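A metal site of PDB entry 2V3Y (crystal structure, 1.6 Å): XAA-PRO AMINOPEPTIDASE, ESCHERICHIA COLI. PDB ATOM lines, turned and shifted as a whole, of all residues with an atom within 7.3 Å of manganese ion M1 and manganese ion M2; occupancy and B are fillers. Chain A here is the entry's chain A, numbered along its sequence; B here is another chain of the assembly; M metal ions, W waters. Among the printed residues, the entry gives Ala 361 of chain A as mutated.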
ATOM      1  N   TYR A 229       9.336  20.239   3.235  1.00  0.00           N
ATOM      2  CA  TYR A 229       9.228  21.520   3.934  1.00  0.00           C
ATOM      3  C   TYR A 229       9.406  21.250   5.424  1.00  0.00           C
ATOM      4  O   TYR A 229       9.329  20.098   5.849  1.00  0.00           O
ATOM      5  CB  TYR A 229       7.912  22.215   3.684  1.00  0.00           C
ATOM      6  CG  TYR A 229       6.719  21.375   4.035  1.00  0.00           C
ATOM      7  CD1 TYR A 229       6.198  20.461   3.096  1.00  0.00           C
ATOM      8  CD2 TYR A 229       6.107  21.448   5.269  1.00  0.00           C
ATOM      9  CE1 TYR A 229       5.132  19.639   3.400  1.00  0.00           C
ATOM     10  CE2 TYR A 229       5.000  20.654   5.583  1.00  0.00           C
ATOM     11  CZ  TYR A 229       4.503  19.722   4.644  1.00  0.00           C
ATOM     12  OH  TYR A 229       3.432  18.906   4.924  1.00  0.00           O
ATOM     13  N   ILE A 232       5.699  20.761  10.857  1.00  0.00           N
ATOM     14  CA  ILE A 232       4.909  21.538  11.810  1.00  0.00           C
ATOM     15  C   ILE A 232       4.244  20.550  12.769  1.00  0.00           C
ATOM     16  O   ILE A 232       3.510  19.673  12.303  1.00  0.00           O
ATOM     17  CB  ILE A 232       3.823  22.330  11.025  1.00  0.00           C
ATOM     18  CG1 ILE A 232       4.480  23.433  10.193  1.00  0.00           C
ATOM     19  CG2 ILE A 232       2.741  22.870  11.952  1.00  0.00           C
ATOM     20  CD1 ILE A 232       3.711  23.809   8.926  1.00  0.00           C
ATOM     21  N   ILE A 259      -0.371  18.221  12.899  1.00  0.00           N
ATOM     22  CA  ILE A 259       0.869  17.843  12.243  1.00  0.00           C
ATOM     23  C   ILE A 259       0.727  18.117  10.751  1.00  0.00           C
ATOM     24  O   ILE A 259      -0.111  17.512  10.109  1.00  0.00           O
ATOM     25  CB  ILE A 259       1.269  16.369  12.474  1.00  0.00           C
ATOM     26  CG1 ILE A 259       1.387  16.095  13.983  1.00  0.00           C
ATOM     27  CG2 ILE A 259       2.570  16.055  11.731  1.00  0.00           C
ATOM     28  CD1 ILE A 259       1.899  14.703  14.300  1.00  0.00           C
ATOM     29  N   ASP A 260       1.568  19.011  10.223  1.00  0.00           N
ATOM     30  CA  ASP A 260       1.633  19.301   8.779  1.00  0.00           C
ATOM     31  C   ASP A 260       3.051  18.898   8.368  1.00  0.00           C
ATOM     32  O   ASP A 260       4.026  19.497   8.825  1.00  0.00           O
ATOM     33  CB  ASP A 260       1.343  20.785   8.529  1.00  0.00           C
ATOM     34  CG  ASP A 260       1.052  21.114   7.054  1.00  0.00           C
ATOM     35  OD1 ASP A 260       1.493  20.350   6.198  1.00  0.00           O
ATOM     36  OD2 ASP A 260       0.409  22.148   6.830  1.00  0.00           O
ATOM     37  N   ALA A 261       3.165  17.780   7.658  1.00  0.00           N
ATOM     38  CA  ALA A 261       4.459  17.214   7.280  1.00  0.00           C
ATOM     39  C   ALA A 261       4.346  16.472   5.985  1.00  0.00           C
ATOM     40  O   ALA A 261       3.320  15.890   5.662  1.00  0.00           O
ATOM     41  CB  ALA A 261       5.001  16.242   8.371  1.00  0.00           C
ATOM     42  N   GLY A 262       5.411  16.540   5.205  1.00  0.00           N
ATOM     43  CA  GLY A 262       5.438  15.886   3.898  1.00  0.00           C
ATOM     44  C   GLY A 262       6.846  15.511   3.474  1.00  0.00           C
ATOM     45  O   GLY A 262       7.806  16.194   3.842  1.00  0.00           O
ATOM     46  N   GLY A 270       5.115  15.266  -0.975  1.00  0.00           N
ATOM     47  CA  GLY A 270       3.905  15.006  -0.241  1.00  0.00           C
ATOM     48  C   GLY A 270       3.592  16.179   0.688  1.00  0.00           C
ATOM     49  O   GLY A 270       4.485  16.958   1.065  1.00  0.00           O
ATOM     50  N   ASP A 271       2.345  16.275   1.148  1.00  0.00           N
ATOM     51  CA  ASP A 271       1.938  17.398   1.981  1.00  0.00           C
ATOM     52  C   ASP A 271       0.626  17.029   2.643  1.00  0.00           C
ATOM     53  O   ASP A 271      -0.450  17.227   2.078  1.00  0.00           O
ATOM     54  CB  ASP A 271       1.812  18.663   1.141  1.00  0.00           C
ATOM     55  CG  ASP A 271       1.350  19.853   1.932  1.00  0.00           C
ATOM     56  OD1 ASP A 271       1.259  19.772   3.186  1.00  0.00           O
ATOM     57  OD2 ASP A 271       1.110  20.908   1.309  1.00  0.00           O
ATOM     58  N   ILE A 272       0.728  16.485   3.858  1.00  0.00           N
ATOM     59  CA  ILE A 272      -0.425  16.056   4.636  1.00  0.00           C
ATOM     60  C   ILE A 272      -0.510  16.813   5.932  1.00  0.00           C
ATOM     61  O   ILE A 272       0.502  17.076   6.594  1.00  0.00           O
ATOM     62  CB  ILE A 272      -0.403  14.526   4.942  1.00  0.00           C
ATOM     63  CG1 ILE A 272      -0.489  13.714   3.633  1.00  0.00           C
ATOM     64  CG2 ILE A 272      -1.551  14.095   5.932  1.00  0.00           C
ATOM     65  CD1 ILE A 272      -0.460  12.194   3.880  1.00  0.00           C
ATOM     66  N   THR A 273      -1.741  17.163   6.311  1.00  0.00           N
ATOM     67  CA  THR A 273      -2.012  17.611   7.675  1.00  0.00           C
ATOM     68  C   THR A 273      -3.054  16.690   8.318  1.00  0.00           C
ATOM     69  O   THR A 273      -4.092  16.372   7.704  1.00  0.00           O
ATOM     70  CB  THR A 273      -2.472  19.074   7.769  1.00  0.00           C
ATOM     71  OG1 THR A 273      -1.592  19.942   7.005  1.00  0.00           O
ATOM     72  CG2 THR A 273      -2.520  19.546   9.269  1.00  0.00           C
ATOM     73  N   LEU A 352      -7.695  27.309   0.498  1.00  0.00           N
ATOM     74  CA  LEU A 352      -8.095  25.909   0.580  1.00  0.00           C
ATOM     75  C   LEU A 352      -7.094  24.963  -0.100  1.00  0.00           C
ATOM     76  O   LEU A 352      -6.954  23.801   0.284  1.00  0.00           O
ATOM     77  CB  LEU A 352      -9.443  25.709  -0.121  1.00  0.00           C
ATOM     78  CG  LEU A 352     -10.052  24.303  -0.089  1.00  0.00           C
ATOM     79  CD1 LEU A 352     -10.366  23.899   1.352  1.00  0.00           C
ATOM     80  CD2 LEU A 352     -11.302  24.272  -0.945  1.00  0.00           C
ATOM     81  N   SER A 353      -6.426  25.456  -1.139  1.00  0.00           N
ATOM     82  CA  SER A 353      -5.648  24.597  -2.023  1.00  0.00           C
ATOM     83  C   SER A 353      -4.458  25.294  -2.649  1.00  0.00           C
ATOM     84  O   SER A 353      -4.539  26.453  -3.036  1.00  0.00           O
ATOM     85  CB  SER A 353      -6.545  24.107  -3.174  1.00  0.00           C
ATOM     86  OG  SER A 353      -7.595  23.265  -2.711  1.00  0.00           O
ATOM     87  N   HIS A 354      -3.367  24.559  -2.794  1.00  0.00           N
ATOM     88  CA  HIS A 354      -2.261  25.014  -3.621  1.00  0.00           C
ATOM     89  C   HIS A 354      -1.812  23.865  -4.516  1.00  0.00           C
ATOM     90  O   HIS A 354      -1.977  22.682  -4.196  1.00  0.00           O
ATOM     91  CB  HIS A 354      -1.085  25.527  -2.768  1.00  0.00           C
ATOM     92  CG  HIS A 354      -0.545  24.527  -1.782  1.00  0.00           C
ATOM     93  ND1 HIS A 354       0.374  23.558  -2.131  1.00  0.00           N
ATOM     94  CD2 HIS A 354      -0.801  24.333  -0.466  1.00  0.00           C
ATOM     95  CE1 HIS A 354       0.661  22.815  -1.070  1.00  0.00           C
ATOM     96  NE2 HIS A 354      -0.056  23.245  -0.048  1.00  0.00           N
ATOM     97  N   TRP A 355      -1.216  24.217  -5.653  1.00  0.00           N
ATOM     98  CA  TRP A 355      -0.585  23.220  -6.519  1.00  0.00           C
ATOM     99  C   TRP A 355       0.482  22.458  -5.779  1.00  0.00           C
ATOM    100  O   TRP A 355       1.113  23.015  -4.858  1.00  0.00           O
ATOM    101  CB  TRP A 355       0.079  23.888  -7.717  1.00  0.00           C
ATOM    102  CG  TRP A 355      -0.762  24.841  -8.522  1.00  0.00           C
ATOM    103  CD1 TRP A 355      -0.374  26.092  -8.909  1.00  0.00           C
ATOM    104  CD2 TRP A 355      -2.055  24.613  -9.129  1.00  0.00           C
ATOM    105  NE1 TRP A 355      -1.343  26.675  -9.684  1.00  0.00           N
ATOM    106  CE2 TRP A 355      -2.400  25.804  -9.828  1.00  0.00           C
ATOM    107  CE3 TRP A 355      -2.970  23.555  -9.110  1.00  0.00           C
ATOM    108  CZ2 TRP A 355      -3.611  25.947 -10.545  1.00  0.00           C
ATOM    109  CZ3 TRP A 355      -4.185  23.709  -9.815  1.00  0.00           C
ATOM    110  CH2 TRP A 355      -4.484  24.895 -10.520  1.00  0.00           C
ATOM    111  N   LEU A 356       0.770  21.225  -6.230  1.00  0.00           N
ATOM    112  CA  LEU A 356       1.752  20.345  -5.572  1.00  0.00           C
ATOM    113  C   LEU A 356       2.654  19.704  -6.644  1.00  0.00           C
ATOM    114  O   LEU A 356       2.138  19.272  -7.695  1.00  0.00           O
ATOM    115  CB  LEU A 356       1.034  19.273  -4.755  1.00  0.00           C
ATOM    116  CG  LEU A 356       1.835  18.319  -3.870  1.00  0.00           C
ATOM    117  CD1 LEU A 356       2.444  19.077  -2.673  1.00  0.00           C
ATOM    118  CD2 LEU A 356       0.911  17.160  -3.386  1.00  0.00           C
ATOM    119  N   VAL A 360       6.527  22.144  -2.875  1.00  0.00           N
ATOM    120  CA  VAL A 360       5.303  21.874  -2.127  1.00  0.00           C
ATOM    121  C   VAL A 360       4.240  22.899  -2.437  1.00  0.00           C
ATOM    122  O   VAL A 360       3.100  22.529  -2.697  1.00  0.00           O
ATOM    123  CB  VAL A 360       5.540  21.710  -0.608  1.00  0.00           C
ATOM    124  CG1 VAL A 360       6.130  22.945   0.016  1.00  0.00           C
ATOM    125  CG2 VAL A 360       4.221  21.281   0.062  1.00  0.00           C
ATOM    126  N   ALA A 361       4.622  24.175  -2.458  1.00  0.00           N
ATOM    127  CA  ALA A 361       3.734  25.237  -2.969  1.00  0.00           C
ATOM    128  C   ALA A 361       4.158  25.392  -4.446  1.00  0.00           C
ATOM    129  O   ALA A 361       5.042  26.171  -4.796  1.00  0.00           O
ATOM    130  CB  ALA A 361       3.868  26.546  -2.174  1.00  0.00           C
ATOM    131  N   THR A 381      -3.423  20.403  -3.238  1.00  0.00           N
ATOM    132  CA  THR A 381      -3.845  20.039  -1.895  1.00  0.00           C
ATOM    133  C   THR A 381      -5.247  20.536  -1.597  1.00  0.00           C
ATOM    134  O   THR A 381      -5.804  21.380  -2.300  1.00  0.00           O
ATOM    135  CB  THR A 381      -2.924  20.640  -0.881  1.00  0.00           C
ATOM    136  OG1 THR A 381      -3.101  22.067  -0.855  1.00  0.00           O
ATOM    137  CG2 THR A 381      -1.439  20.215  -1.183  1.00  0.00           C
ATOM    138  N   VAL A 382      -5.822  19.978  -0.532  1.00  0.00           N
ATOM    139  CA  VAL A 382      -7.151  20.395  -0.050  1.00  0.00           C
ATOM    140  C   VAL A 382      -6.965  20.459   1.468  1.00  0.00           C
ATOM    141  O   VAL A 382      -6.750  19.415   2.107  1.00  0.00           O
ATOM    142  CB  VAL A 382      -8.255  19.393  -0.428  1.00  0.00           C
ATOM    143  CG1 VAL A 382      -9.649  19.940  -0.087  1.00  0.00           C
ATOM    144  CG2 VAL A 382      -8.139  19.035  -1.920  1.00  0.00           C
ATOM    145  N   GLU A 383      -6.975  21.674   2.013  1.00  0.00           N
ATOM    146  CA  GLU A 383      -6.533  21.900   3.390  1.00  0.00           C
ATOM    147  C   GLU A 383      -7.368  22.922   4.144  1.00  0.00           C
ATOM    148  O   GLU A 383      -6.845  23.920   4.641  1.00  0.00           O
ATOM    149  CB  GLU A 383      -5.039  22.246   3.438  1.00  0.00           C
ATOM    150  CG  GLU A 383      -4.577  23.452   2.694  1.00  0.00           C
ATOM    151  CD  GLU A 383      -3.054  23.541   2.767  1.00  0.00           C
ATOM    152  OE1 GLU A 383      -2.469  23.614   3.880  1.00  0.00           O
ATOM    153  OE2 GLU A 383      -2.460  23.451   1.677  1.00  0.00           O
ATOM    154  N   ARG A 404      -6.467  21.554  11.249  1.00  0.00           N
ATOM    155  CA  ARG A 404      -6.365  21.520   9.805  1.00  0.00           C
ATOM    156  C   ARG A 404      -6.299  20.059   9.388  1.00  0.00           C
ATOM    157  O   ARG A 404      -5.714  19.236  10.077  1.00  0.00           O
ATOM    158  CB  ARG A 404      -5.110  22.271   9.319  1.00  0.00           C
ATOM    159  CG  ARG A 404      -4.919  22.244   7.795  1.00  0.00           C
ATOM    160  CD  ARG A 404      -3.900  23.279   7.289  1.00  0.00           C
ATOM    161  NE  ARG A 404      -2.521  23.117   7.777  1.00  0.00           N
ATOM    162  CZ  ARG A 404      -1.946  23.848   8.740  1.00  0.00           C
ATOM    163  NH1 ARG A 404      -2.622  24.756   9.423  1.00  0.00           N
ATOM    164  NH2 ARG A 404      -0.660  23.662   9.048  1.00  0.00           N
ATOM    165  N   GLU A 406      -5.631  17.899   5.765  1.00  0.00           N
ATOM    166  CA  GLU A 406      -5.178  18.130   4.398  1.00  0.00           C
ATOM    167  C   GLU A 406      -4.835  16.828   3.698  1.00  0.00           C
ATOM    168  O   GLU A 406      -4.068  16.010   4.229  1.00  0.00           O
ATOM    169  CB  GLU A 406      -3.958  19.042   4.425  1.00  0.00           C
ATOM    170  CG  GLU A 406      -3.175  19.142   3.120  1.00  0.00           C
ATOM    171  CD  GLU A 406      -2.011  20.112   3.224  1.00  0.00           C
ATOM    172  OE1 GLU A 406      -1.444  20.271   4.313  1.00  0.00           O
ATOM    173  OE2 GLU A 406      -1.685  20.704   2.190  1.00  0.00           O
ATOM    174  N   ASP A 407      -5.379  16.698   2.471  1.00  0.00           N
ATOM    175  CA  ASP A 407      -5.052  15.619   1.544  1.00  0.00           C
ATOM    176  C   ASP A 407      -4.463  16.217   0.242  1.00  0.00           C
ATOM    177  O   ASP A 407      -4.653  17.412  -0.039  1.00  0.00           O
ATOM    178  CB  ASP A 407      -6.297  14.799   1.192  1.00  0.00           C
ATOM    179  CG  ASP A 407      -6.650  13.748   2.258  1.00  0.00           C
ATOM    180  OD1 ASP A 407      -5.718  13.320   3.016  1.00  0.00           O
ATOM    181  OD2 ASP A 407      -7.838  13.379   2.323  1.00  0.00           O
ATOM    182  N   ASP A 408      -3.771  15.362  -0.505  1.00  0.00           N
ATOM    183  CA  ASP A 408      -3.203  15.689  -1.817  1.00  0.00           C
ATOM    184  C   ASP A 408      -4.007  14.914  -2.856  1.00  0.00           C
ATOM    185  O   ASP A 408      -4.222  13.704  -2.707  1.00  0.00           O
ATOM    186  CB  ASP A 408      -1.736  15.270  -1.905  1.00  0.00           C
ATOM    187  CG  ASP A 408      -0.921  15.847  -0.782  1.00  0.00           C
ATOM    188  OD1 ASP A 408      -1.290  16.954  -0.289  1.00  0.00           O
ATOM    189  OD2 ASP A 408       0.058  15.168  -0.368  1.00  0.00           O
ATOM    190  N   PRO B   2       0.216  26.112   4.647  1.00  0.00           N
ATOM    191  CA  PRO B   2      -0.933  26.716   3.947  1.00  0.00           C
ATOM    192  C   PRO B   2      -0.535  27.925   3.096  1.00  0.00           C
ATOM    193  O   PRO B   2       0.433  28.626   3.441  1.00  0.00           O
ATOM    194  CB  PRO B   2      -1.844  27.164   5.091  1.00  0.00           C
ATOM    195  CG  PRO B   2      -1.501  26.251   6.247  1.00  0.00           C
ATOM    196  CD  PRO B   2      -0.110  25.738   6.038  1.00  0.00           C
ATOM    197  N   LEU B   3      -1.264  28.154   2.005  1.00  0.00           N
ATOM    198  CA  LEU B   3      -1.001  29.312   1.139  1.00  0.00           C
ATOM    199  C   LEU B   3      -2.001  30.443   1.426  1.00  0.00           C
ATOM    200  O   LEU B   3      -1.666  31.626   1.324  1.00  0.00           O
ATOM    201  CB  LEU B   3      -1.057  28.942  -0.351  1.00  0.00           C
ATOM    202  CG  LEU B   3       0.207  28.997  -1.232  1.00  0.00           C
ATOM    203  CD1 LEU B   3      -0.187  29.107  -2.712  1.00  0.00           C
ATOM    204  CD2 LEU B   3       1.169  30.122  -0.862  1.00  0.00           C
ATOM    205  OXT LEU B   3      -3.149  30.219   1.751  1.00  0.00           O
HETATM  206 MN    MN M   1      -0.402  22.305   1.792  1.00  0.00          MN
HETATM  207 MN    MN M   2       0.430  21.129   4.425  1.00  0.00          MN
HETATM  208  O   HOH W   1       0.176  22.696   3.696  1.00  0.00           O
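OH of Tyr 229 touches manganese ion M2 (3.8 Å). Thr 273 touches manganese ion M2 (OG1 to MN, 3.5 Å). Six residues have an atom within 4 Å of manganese ion M2: Tyr 229, Asp 260, Asp 271, Thr 273, Glu 383 and Glu 406.
Manganese ion M1 is bound by water W1 (2.0 Å), the side-chain carboxylate of Glu 406 (2.1 Å), a ring nitrogen (NE2) of His 354 (2.1 Å), the side-chain carboxylate of Asp 271 (2.1 Å) and the side-chain carboxylate of Glu 383 (2.4 Å). Manganese ion M1 has five donor atoms within binding distance.
The side-chain carboxylate of Asp 271 sits close to the side-chain hydroxyl of Tyr 229 (2.9 Å). N of Asp 271 lies within hydrogen-bond range of OD2 of Asp 408 (3.0 Å). A ring nitrogen (ND1) of His 354 lies close to the backbone carbonyl oxygen of Val 360, 3.0 Å away. OG1 of Thr 273 sits close to OD2 of Asp 260. OD1 of Asp 260 sits close to OH of Tyr 229 (2.7 Å). OE1 of Glu 383 lies within salt-bridge range of NE of Arg 404 (3.9 Å). NE of Arg 404 lies within hydrogen-bond range of OG1 of Thr 273 (3.4 Å). The backbone NH (N) of Ala 261 lies close to the side-chain hydroxyl (OH) of Tyr 229 (3.0 Å).
Merely in contact with manganese ion M1: Thr 381. Along chain A the residues within 4 Å of manganese ion M1 span positions 271 to 406. The nearest printed residue that does not touch manganese ion M1 is Pro 2 of chain B (4.8 Å).
Manganese ion M2 is bound by water W1, the side-chain carboxylate (OD1) of Asp 271, the side-chain carboxylate (OE1) of Glu 406, the side-chain carboxylate (OD1) of Asp 260 and the side-chain carboxylate (OD2) of Asp 260. Manganese ion M2 has five donor atoms within binding distance.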
